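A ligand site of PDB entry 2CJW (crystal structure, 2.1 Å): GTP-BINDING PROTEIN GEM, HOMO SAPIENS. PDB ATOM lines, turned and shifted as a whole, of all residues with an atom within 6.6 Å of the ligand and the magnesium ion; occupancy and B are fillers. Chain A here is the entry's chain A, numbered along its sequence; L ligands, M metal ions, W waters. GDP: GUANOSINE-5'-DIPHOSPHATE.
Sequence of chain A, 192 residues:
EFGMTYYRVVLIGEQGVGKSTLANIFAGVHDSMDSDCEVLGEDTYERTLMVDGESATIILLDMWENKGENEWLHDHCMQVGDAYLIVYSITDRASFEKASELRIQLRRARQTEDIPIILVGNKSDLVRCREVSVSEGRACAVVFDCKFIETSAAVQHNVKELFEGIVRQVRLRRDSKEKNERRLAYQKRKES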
ATOM      1  N   GLY A  13      -3.467  23.295 -32.534  1.00  0.00           N
ATOM      2  CA  GLY A  13      -4.052  21.965 -32.683  1.00  0.00           C
ATOM      3  C   GLY A  13      -5.192  21.973 -33.668  1.00  0.00           C
ATOM      4  O   GLY A  13      -5.686  23.054 -34.023  1.00  0.00           O
ATOM      5  N   GLU A  14      -5.621  20.791 -34.102  1.00  0.00           N
ATOM      6  CA  GLU A  14      -6.750  20.670 -35.027  1.00  0.00           C
ATOM      7  C   GLU A  14      -8.035  21.311 -34.509  1.00  0.00           C
ATOM      8  O   GLU A  14      -8.262  21.378 -33.297  1.00  0.00           O
ATOM      9  CB  GLU A  14      -7.020  19.119 -35.177  1.00  0.00           C
ATOM     10  CG  GLU A  14      -8.379  18.593 -35.918  1.00  0.00           C
ATOM     11  CD  GLU A  14      -8.231  17.236 -36.690  1.00  0.00           C
ATOM     12  OE1 GLU A  14      -7.495  17.149 -37.709  1.00  0.00           O
ATOM     13  OE2 GLU A  14      -8.918  16.273 -36.303  1.00  0.00           O
ATOM     14  N   GLN A  15      -8.831  21.856 -35.433  1.00  0.00           N
ATOM     15  CA  GLN A  15     -10.139  22.386 -35.079  1.00  0.00           C
ATOM     16  C   GLN A  15     -10.952  21.336 -34.334  1.00  0.00           C
ATOM     17  O   GLN A  15     -11.001  20.162 -34.726  1.00  0.00           O
ATOM     18  CB  GLN A  15     -10.898  22.894 -36.308  1.00  0.00           C
ATOM     19  CG  GLN A  15     -12.211  23.628 -35.937  1.00  0.00           C
ATOM     20  CD  GLN A  15     -12.884  24.329 -37.121  1.00  0.00           C
ATOM     21  OE1 GLN A  15     -12.560  24.069 -38.278  1.00  0.00           O
ATOM     22  NE2 GLN A  15     -13.817  25.215 -36.817  1.00  0.00           N
ATOM     23  N   GLY A  16     -11.580  21.767 -33.238  1.00  0.00           N
ATOM     24  CA  GLY A  16     -12.527  20.933 -32.506  1.00  0.00           C
ATOM     25  C   GLY A  16     -11.938  20.132 -31.352  1.00  0.00           C
ATOM     26  O   GLY A  16     -12.647  19.352 -30.721  1.00  0.00           O
ATOM     27  N   VAL A  17     -10.646  20.313 -31.069  1.00  0.00           N
ATOM     28  CA  VAL A  17      -9.999  19.514 -30.005  1.00  0.00           C
ATOM     29  C   VAL A  17     -10.253  20.112 -28.590  1.00  0.00           C
ATOM     30  O   VAL A  17     -10.013  19.442 -27.590  1.00  0.00           O
ATOM     31  CB  VAL A  17      -8.479  19.307 -30.228  1.00  0.00           C
ATOM     32  CG1 VAL A  17      -8.179  18.535 -31.554  1.00  0.00           C
ATOM     33  CG2 VAL A  17      -7.734  20.633 -30.183  1.00  0.00           C
ATOM     34  N   GLY A  18     -10.726  21.356 -28.535  1.00  0.00           N
ATOM     35  CA  GLY A  18     -11.058  22.020 -27.265  1.00  0.00           C
ATOM     36  C   GLY A  18     -10.141  23.154 -26.844  1.00  0.00           C
ATOM     37  O   GLY A  18     -10.121  23.528 -25.662  1.00  0.00           O
ATOM     38  N   LYS A  19      -9.398  23.746 -27.786  1.00  0.00           N
ATOM     39  CA  LYS A  19      -8.519  24.873 -27.492  1.00  0.00           C
ATOM     40  C   LYS A  19      -9.295  26.064 -26.883  1.00  0.00           C
ATOM     41  O   LYS A  19      -8.889  26.589 -25.839  1.00  0.00           O
ATOM     42  CB  LYS A  19      -7.743  25.323 -28.725  1.00  0.00           C
ATOM     43  CG  LYS A  19      -6.841  24.206 -29.316  1.00  0.00           C
ATOM     44  CD  LYS A  19      -6.051  24.683 -30.563  1.00  0.00           C
ATOM     45  CE  LYS A  19      -6.948  25.169 -31.726  1.00  0.00           C
ATOM     46  NZ  LYS A  19      -7.945  24.195 -32.241  1.00  0.00           N
ATOM     47  N   SER A  20     -10.396  26.437 -27.512  1.00  0.00           N
ATOM     48  CA  SER A  20     -11.176  27.612 -27.040  1.00  0.00           C
ATOM     49  C   SER A  20     -11.862  27.361 -25.697  1.00  0.00           C
ATOM     50  O   SER A  20     -11.980  28.272 -24.865  1.00  0.00           O
ATOM     51  CB  SER A  20     -12.177  28.019 -28.101  1.00  0.00           C
ATOM     52  OG  SER A  20     -11.479  28.632 -29.173  1.00  0.00           O
ATOM     53  N   THR A  21     -12.306  26.133 -25.508  1.00  0.00           N
ATOM     54  CA  THR A  21     -12.966  25.681 -24.283  1.00  0.00           C
ATOM     55  C   THR A  21     -11.953  25.677 -23.132  1.00  0.00           C
ATOM     56  O   THR A  21     -12.240  26.213 -22.062  1.00  0.00           O
ATOM     57  CB  THR A  21     -13.660  24.303 -24.464  1.00  0.00           C
ATOM     58  OG1 THR A  21     -14.530  24.358 -25.601  1.00  0.00           O
ATOM     59  CG2 THR A  21     -14.504  23.920 -23.241  1.00  0.00           C
ATOM     60  N   LEU A  22     -10.765  25.112 -23.351  1.00  0.00           N
ATOM     61  CA  LEU A  22      -9.669  25.239 -22.388  1.00  0.00           C
ATOM     62  C   LEU A  22      -9.341  26.700 -22.008  1.00  0.00           C
ATOM     63  O   LEU A  22      -9.249  27.051 -20.804  1.00  0.00           O
ATOM     64  CB  LEU A  22      -8.403  24.541 -22.909  1.00  0.00           C
ATOM     65  CG  LEU A  22      -8.393  23.004 -22.781  1.00  0.00           C
ATOM     66  CD1 LEU A  22      -7.330  22.387 -23.707  1.00  0.00           C
ATOM     67  CD2 LEU A  22      -8.144  22.573 -21.321  1.00  0.00           C
ATOM     68  N   ASP A  43      -9.711  36.576 -28.759  1.00  0.00           N
ATOM     69  CA  ASP A  43      -8.988  35.289 -28.688  1.00  0.00           C
ATOM     70  C   ASP A  43      -7.704  35.337 -27.832  1.00  0.00           C
ATOM     71  O   ASP A  43      -6.895  34.413 -27.873  1.00  0.00           O
ATOM     72  CB  ASP A  43      -8.720  34.752 -30.092  1.00  0.00           C
ATOM     73  CG  ASP A  43     -10.004  34.500 -30.866  1.00  0.00           C
ATOM     74  OD1 ASP A  43     -10.929  33.859 -30.312  1.00  0.00           O
ATOM     75  OD2 ASP A  43     -10.086  34.934 -32.033  1.00  0.00           O
ATOM     76  N   ASP A  62      -5.252  32.185 -28.323  1.00  0.00           N
ATOM     77  CA  ASP A  62      -6.081  31.167 -28.947  1.00  0.00           C
ATOM     78  C   ASP A  62      -6.580  31.599 -30.338  1.00  0.00           C
ATOM     79  O   ASP A  62      -7.766  31.565 -30.632  1.00  0.00           O
ATOM     80  CB  ASP A  62      -7.269  30.845 -28.012  1.00  0.00           C
ATOM     81  CG  ASP A  62      -8.248  29.850 -28.608  1.00  0.00           C
ATOM     82  OD1 ASP A  62      -7.800  28.842 -29.211  1.00  0.00           O
ATOM     83  OD2 ASP A  62      -9.474  30.075 -28.471  1.00  0.00           O
ATOM     84  N   GLU A  65      -7.248  29.139 -35.458  1.00  0.00           N
ATOM     85  CA  GLU A  65      -8.266  28.941 -36.504  1.00  0.00           C
ATOM     86  C   GLU A  65      -8.274  30.081 -37.533  1.00  0.00           C
ATOM     87  O   GLU A  65      -8.158  31.261 -37.174  1.00  0.00           O
ATOM     88  CB  GLU A  65      -9.655  28.780 -35.888  1.00  0.00           C
ATOM     89  CG  GLU A  65     -10.743  28.305 -36.860  1.00  0.00           C
ATOM     90  CD  GLU A  65     -12.157  28.481 -36.321  1.00  0.00           C
ATOM     91  OE1 GLU A  65     -12.410  28.152 -35.132  1.00  0.00           O
ATOM     92  OE2 GLU A  65     -13.034  28.930 -37.083  1.00  0.00           O
ATOM     93  N   VAL A  87      -2.448  20.653 -28.649  1.00  0.00           N
ATOM     94  CA  VAL A  87      -3.617  19.942 -28.146  1.00  0.00           C
ATOM     95  C   VAL A  87      -4.186  19.012 -29.189  1.00  0.00           C
ATOM     96  O   VAL A  87      -4.346  19.376 -30.356  1.00  0.00           O
ATOM     97  CB  VAL A  87      -4.734  20.953 -27.725  1.00  0.00           C
ATOM     98  CG1 VAL A  87      -5.903  20.224 -27.010  1.00  0.00           C
ATOM     99  CG2 VAL A  87      -4.136  22.073 -26.853  1.00  0.00           C
ATOM    100  N   ASN A 122      -6.617  16.327 -24.701  1.00  0.00           N
ATOM    101  CA  ASN A 122      -7.847  16.883 -24.123  1.00  0.00           C
ATOM    102  C   ASN A 122      -9.043  15.953 -24.320  1.00  0.00           C
ATOM    103  O   ASN A 122      -8.990  15.011 -25.107  1.00  0.00           O
ATOM    104  CB  ASN A 122      -8.096  18.301 -24.676  1.00  0.00           C
ATOM    105  CG  ASN A 122      -9.227  19.050 -23.941  1.00  0.00           C
ATOM    106  OD1 ASN A 122      -9.266  19.104 -22.709  1.00  0.00           O
ATOM    107  ND2 ASN A 122     -10.156  19.602 -24.704  1.00  0.00           N
ATOM    108  N   LYS A 123     -10.136  16.229 -23.598  1.00  0.00           N
ATOM    109  CA  LYS A 123     -11.362  15.429 -23.611  1.00  0.00           C
ATOM    110  C   LYS A 123     -11.191  14.090 -22.889  1.00  0.00           C
ATOM    111  O   LYS A 123     -11.828  13.096 -23.249  1.00  0.00           O
ATOM    112  CB  LYS A 123     -11.957  15.273 -25.036  1.00  0.00           C
ATOM    113  CG  LYS A 123     -12.039  16.570 -25.847  1.00  0.00           C
ATOM    114  CD  LYS A 123     -13.006  16.451 -27.019  1.00  0.00           C
ATOM    115  CE  LYS A 123     -13.020  17.695 -27.889  1.00  0.00           C
ATOM    116  NZ  LYS A 123     -14.084  17.597 -28.931  1.00  0.00           N
ATOM    117  N   SER A 124     -10.359  14.074 -21.845  1.00  0.00           N
ATOM    118  CA  SER A 124     -10.108  12.872 -21.033  1.00  0.00           C
ATOM    119  C   SER A 124     -11.370  12.251 -20.387  1.00  0.00           C
ATOM    120  O   SER A 124     -11.379  11.072 -20.007  1.00  0.00           O
ATOM    121  CB  SER A 124      -9.047  13.171 -19.946  1.00  0.00           C
ATOM    122  OG  SER A 124      -9.607  13.975 -18.902  1.00  0.00           O
ATOM    123  N   ASP A 125     -12.441  13.043 -20.308  1.00  0.00           N
ATOM    124  CA  ASP A 125     -13.732  12.585 -19.760  1.00  0.00           C
ATOM    125  C   ASP A 125     -14.462  11.635 -20.728  1.00  0.00           C
ATOM    126  O   ASP A 125     -15.352  10.894 -20.314  1.00  0.00           O
ATOM    127  CB  ASP A 125     -14.618  13.797 -19.440  1.00  0.00           C
ATOM    128  CG  ASP A 125     -14.864  14.702 -20.655  1.00  0.00           C
ATOM    129  OD1 ASP A 125     -13.917  15.363 -21.137  1.00  0.00           O
ATOM    130  OD2 ASP A 125     -16.009  14.743 -21.130  1.00  0.00           O
ATOM    131  N   LEU A 126     -14.095  11.659 -22.008  1.00  0.00           N
ATOM    132  CA  LEU A 126     -14.774  10.819 -22.985  1.00  0.00           C
ATOM    133  C   LEU A 126     -14.102   9.452 -23.109  1.00  0.00           C
ATOM    134  O   LEU A 126     -13.644   9.069 -24.187  1.00  0.00           O
ATOM    135  CB  LEU A 126     -14.875  11.531 -24.341  1.00  0.00           C
ATOM    136  CG  LEU A 126     -15.525  12.922 -24.288  1.00  0.00           C
ATOM    137  CD1 LEU A 126     -15.480  13.601 -25.659  1.00  0.00           C
ATOM    138  CD2 LEU A 126     -16.959  12.839 -23.748  1.00  0.00           C
ATOM    139  N   CAS A 129     -14.919   6.734 -25.818  1.00  0.00           N
ATOM    140  CA  CAS A 129     -14.637   7.076 -27.221  1.00  0.00           C
ATOM    141  CB  CAS A 129     -15.431   8.346 -27.565  1.00  0.00           C
ATOM    142  C   CAS A 129     -13.160   7.241 -27.509  1.00  0.00           C
ATOM    143  O   CAS A 129     -12.792   7.731 -28.579  1.00  0.00           O
ATOM    144  SG  CAS A 129     -17.124   7.895 -27.761  1.00  0.00           S
ATOM    145 AS   CAS A 129     -17.959   9.221 -26.183  1.00  0.00          AS
ATOM    146  CE1 CAS A 129     -18.139   8.645 -24.295  1.00  0.00           C
ATOM    147  CE2 CAS A 129     -18.501  11.039 -26.779  1.00  0.00           C
ATOM    148  N   THR A 151      -6.030  16.172 -20.184  1.00  0.00           N
ATOM    149  CA  THR A 151      -6.908  17.203 -19.580  1.00  0.00           C
ATOM    150  C   THR A 151      -8.364  17.000 -19.980  1.00  0.00           C
ATOM    151  O   THR A 151      -8.668  16.290 -20.955  1.00  0.00           O
ATOM    152  CB  THR A 151      -6.524  18.644 -20.024  1.00  0.00           C
ATOM    153  OG1 THR A 151      -6.690  18.785 -21.452  1.00  0.00           O
ATOM    154  CG2 THR A 151      -5.102  19.011 -19.636  1.00  0.00           C
ATOM    155  N   SER A 152      -9.256  17.645 -19.230  1.00  0.00           N
ATOM    156  CA  SER A 152     -10.618  17.821 -19.642  1.00  0.00           C
ATOM    157  C   SER A 152     -11.078  19.223 -19.282  1.00  0.00           C
ATOM    158  O   SER A 152     -11.137  19.576 -18.095  1.00  0.00           O
ATOM    159  CB  SER A 152     -11.548  16.777 -18.993  1.00  0.00           C
ATOM    160  OG  SER A 152     -12.886  16.997 -19.417  1.00  0.00           O
ATOM    161  N   ALA A 153     -11.384  20.007 -20.311  1.00  0.00           N
ATOM    162  CA  ALA A 153     -12.029  21.294 -20.110  1.00  0.00           C
ATOM    163  C   ALA A 153     -13.478  21.105 -19.627  1.00  0.00           C
ATOM    164  O   ALA A 153     -13.994  21.950 -18.890  1.00  0.00           O
ATOM    165  CB  ALA A 153     -11.980  22.146 -21.381  1.00  0.00           C
ATOM    166  N   ALA A 154     -14.117  19.995 -20.032  1.00  0.00           N
ATOM    167  CA  ALA A 154     -15.513  19.740 -19.651  1.00  0.00           C
ATOM    168  C   ALA A 154     -15.675  19.450 -18.161  1.00  0.00           C
ATOM    169  O   ALA A 154     -16.705  19.761 -17.577  1.00  0.00           O
ATOM    170  CB  ALA A 154     -16.105  18.591 -20.469  1.00  0.00           C
ATOM    171  N   VAL A 155     -14.637  18.904 -17.555  1.00  0.00           N
ATOM    172  CA  VAL A 155     -14.726  18.348 -16.213  1.00  0.00           C
ATOM    173  C   VAL A 155     -13.704  19.021 -15.291  1.00  0.00           C
ATOM    174  O   VAL A 155     -13.658  18.773 -14.070  1.00  0.00           O
ATOM    175  CB  VAL A 155     -14.576  16.815 -16.388  1.00  0.00           C
ATOM    176  CG1 VAL A 155     -13.412  16.198 -15.642  1.00  0.00           C
ATOM    177  CG2 VAL A 155     -15.901  16.144 -16.240  1.00  0.00           C
HETATM  178  PB  GDP L   1     -11.322  24.268 -30.801  1.00  0.00           P
HETATM  179  O1B GDP L   1     -11.737  24.283 -32.247  1.00  0.00           O
HETATM  180  O2B GDP L   1     -11.168  25.669 -30.312  1.00  0.00           O
HETATM  181  O3B GDP L   1     -10.025  23.549 -30.600  1.00  0.00           O
HETATM  182  O3A GDP L   1     -12.451  23.429 -30.027  1.00  0.00           O
HETATM  183  PA  GDP L   1     -13.617  24.051 -29.086  1.00  0.00           P
HETATM  184  O1A GDP L   1     -13.034  24.671 -27.857  1.00  0.00           O
HETATM  185  O2A GDP L   1     -14.477  24.975 -29.874  1.00  0.00           O
HETATM  186  O5' GDP L   1     -14.384  22.690 -28.747  1.00  0.00           O
HETATM  187  C5' GDP L   1     -15.084  21.898 -29.719  1.00  0.00           C
HETATM  188  C4' GDP L   1     -16.157  21.062 -29.035  1.00  0.00           C
HETATM  189  O4' GDP L   1     -15.587  20.174 -28.065  1.00  0.00           O
HETATM  190  C3' GDP L   1     -17.159  21.930 -28.271  1.00  0.00           C
HETATM  191  O3' GDP L   1     -18.428  21.317 -28.429  1.00  0.00           O
HETATM  192  C2' GDP L   1     -16.742  21.819 -26.812  1.00  0.00           C
HETATM  193  O2' GDP L   1     -17.853  21.900 -25.934  1.00  0.00           O
HETATM  194  C1' GDP L   1     -16.161  20.421 -26.767  1.00  0.00           C
HETATM  195  N9  GDP L   1     -15.106  20.219 -25.764  1.00  0.00           N
HETATM  196  C8  GDP L   1     -14.004  20.972 -25.575  1.00  0.00           C
HETATM  197  N7  GDP L   1     -13.252  20.441 -24.597  1.00  0.00           N
HETATM  198  C5  GDP L   1     -13.858  19.318 -24.165  1.00  0.00           C
HETATM  199  C6  GDP L   1     -13.600  18.281 -23.133  1.00  0.00           C
HETATM  200  O6  GDP L   1     -12.591  18.306 -22.406  1.00  0.00           O
HETATM  201  N1  GDP L   1     -14.510  17.302 -23.022  1.00  0.00           N
HETATM  202  C2  GDP L   1     -15.616  17.221 -23.767  1.00  0.00           C
HETATM  203  N2  GDP L   1     -16.463  16.198 -23.543  1.00  0.00           N
HETATM  204  N3  GDP L   1     -15.919  18.142 -24.720  1.00  0.00           N
HETATM  205  C4  GDP L   1     -15.084  19.184 -24.934  1.00  0.00           C
HETATM  206 MG    MG M   1     -11.502  27.490 -31.060  1.00  0.00          MG
HETATM  207  O   HOH W   1     -17.848  24.803 -25.807  1.00  0.00           O
HETATM  208  O   HOH W   2     -18.783  15.826 -25.562  1.00  0.00           O
HETATM  209  O   HOH W   3     -11.369  26.799 -33.085  1.00  0.00           O
HETATM  210  O   HOH W   4     -20.539  22.921 -28.050  1.00  0.00           O
HETATM  211  O   HOH W   5     -13.591  27.290 -30.926  1.00  0.00           O
HETATM  212  O   HOH W   6     -16.617  17.066 -27.843  1.00  0.00           O
HETATM  213  O   HOH W   7      -9.507  27.867 -31.165  1.00  0.00           O
HETATM  214  O   HOH W   8     -18.791  18.618 -28.603  1.00  0.00           O
HETATM  215  O   HOH W   9     -11.730  29.524 -32.026  1.00  0.00           O
HETATM  216  O   HOH W  10     -14.208  24.096 -33.100  1.00  0.00           O
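O of Glu 14 touches O3B of the ligand, at 3.9 Å. Gln 15 touches the ligand (C to O1B, 3.7 Å). Leu 126 touches the ligand (CD2 to N2, 3.4 Å). Hydrophobic or aromatic side chains that line the ligand: Val 17, Leu 126, Ala 153 and Ala 154. 15 residues have an atom within 4 Å of the ligand: Glu 14, Gln 15, Gly 16, Val 17, Gly 18, Lys 19, Ser 20, Thr 21, Asn 122, Lys 123, Asp 125, Leu 126, Ser 152, Ala 153 and Ala 154.
OD2 of Asp 62 sits close to OG of Ser 20 (2.6 Å). O of Gly 16 lies within hydrogen-bond range of NZ of Lys 123. The side-chain amino group of Lys 19 is in hydrogen-bond range of the backbone carbonyl oxygen of Glu 14 (3.0 Å). The backbone NH of Ala 153 is in hydrogen-bond range of the side-chain amide oxygen of Asn 122. O of Val 17 sits at hydrogen-bond distance from ND2 of Asn 122 (2.9 Å). The side-chain hydroxyl (OG1) of Thr 151 sits at hydrogen-bond distance from the side-chain amide oxygen (OD1) of Asn 122 (2.9 Å). The backbone NH (N) of Ala 154 lies close to the side-chain hydroxyl (OG) of Ser 152, 3.3 Å away. The backbone NH (N) of Val 155 lies within hydrogen-bond range of the side-chain hydroxyl (OG) of Ser 152 (3.2 Å).
The magnesium ion is bound by O2B of the ligand (2.0 Å), water W7 (2.0 Å), water W5 (2.1 Å), water W3 (2.1 Å), OG of Ser 20 (2.2 Å) and water W9 (2.3 Å). The magnesium ion has six donor atoms within binding distance.
One residue has an atom within 4 Å of the magnesium ion: Ser 20. The nearest printed residue that does not touch the magnesium ion is Asp 62 (4.2 Å).
The backbone NH (N) of Ser 20 is in hydrogen-bond range of an oxygen (O1A) of the ligand (3.2 Å). N of Gly 16 is in hydrogen-bond range of O1B of the ligand. O1A of the ligand is in hydrogen-bond range of N of Thr 21, 2.9 Å away. O1A of the ligand is in hydrogen-bond range of OG1 of Thr 21 (2.7 Å). O3B of the ligand lies within hydrogen-bond range of N of Lys 19 (2.9 Å). The side-chain amino group of Lys 19 is in salt-bridge range of an oxygen (O3B) of the ligand, 2.7 Å away. The side-chain carboxylate of Asp 125 is in hydrogen-bond range of a nitrogen (N1) of the ligand (2.8 Å). An oxygen (O6) of the ligand sits at hydrogen-bond distance from the backbone NH (N) of Ala 153 (3.0 Å). An oxygen (O3A) of the ligand is in hydrogen-bond range of the backbone NH (N) of Gly 18. The backbone NH (N) of Lys 123 sits close to an oxygen (O6) of the ligand, 3.4 Å away. NZ of Lys 123 is in hydrogen-bond range of O4' of the ligand (3.1 Å). ND2 of Asn 122 is in hydrogen-bond range of N7 of the ligand, at 3.2 Å. The backbone NH (N) of Ala 154 sits at hydrogen-bond distance from an oxygen (O6) of the ligand (3.3 Å). O6 of the ligand is in hydrogen-bond range of OG of Ser 152 (3.3 Å). N of Val 17 lies within hydrogen-bond range of O3B of the ligand, at 3.3 Å.
Water W3 bridges OE1 of Glu 65 (2.7 Å) and O1B of the ligand (2.7 Å). Water W1 bridges an oxygen (O2') of the ligand (2.9 Å) and the side-chain hydroxyl of Thr 21 (3.4 Å). Water W6 lies within hydrogen-bond range of the side-chain amino group (NZ) of Lys 123 (2.8 Å) and an oxygen (O4') of the ligand (3.3 Å).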
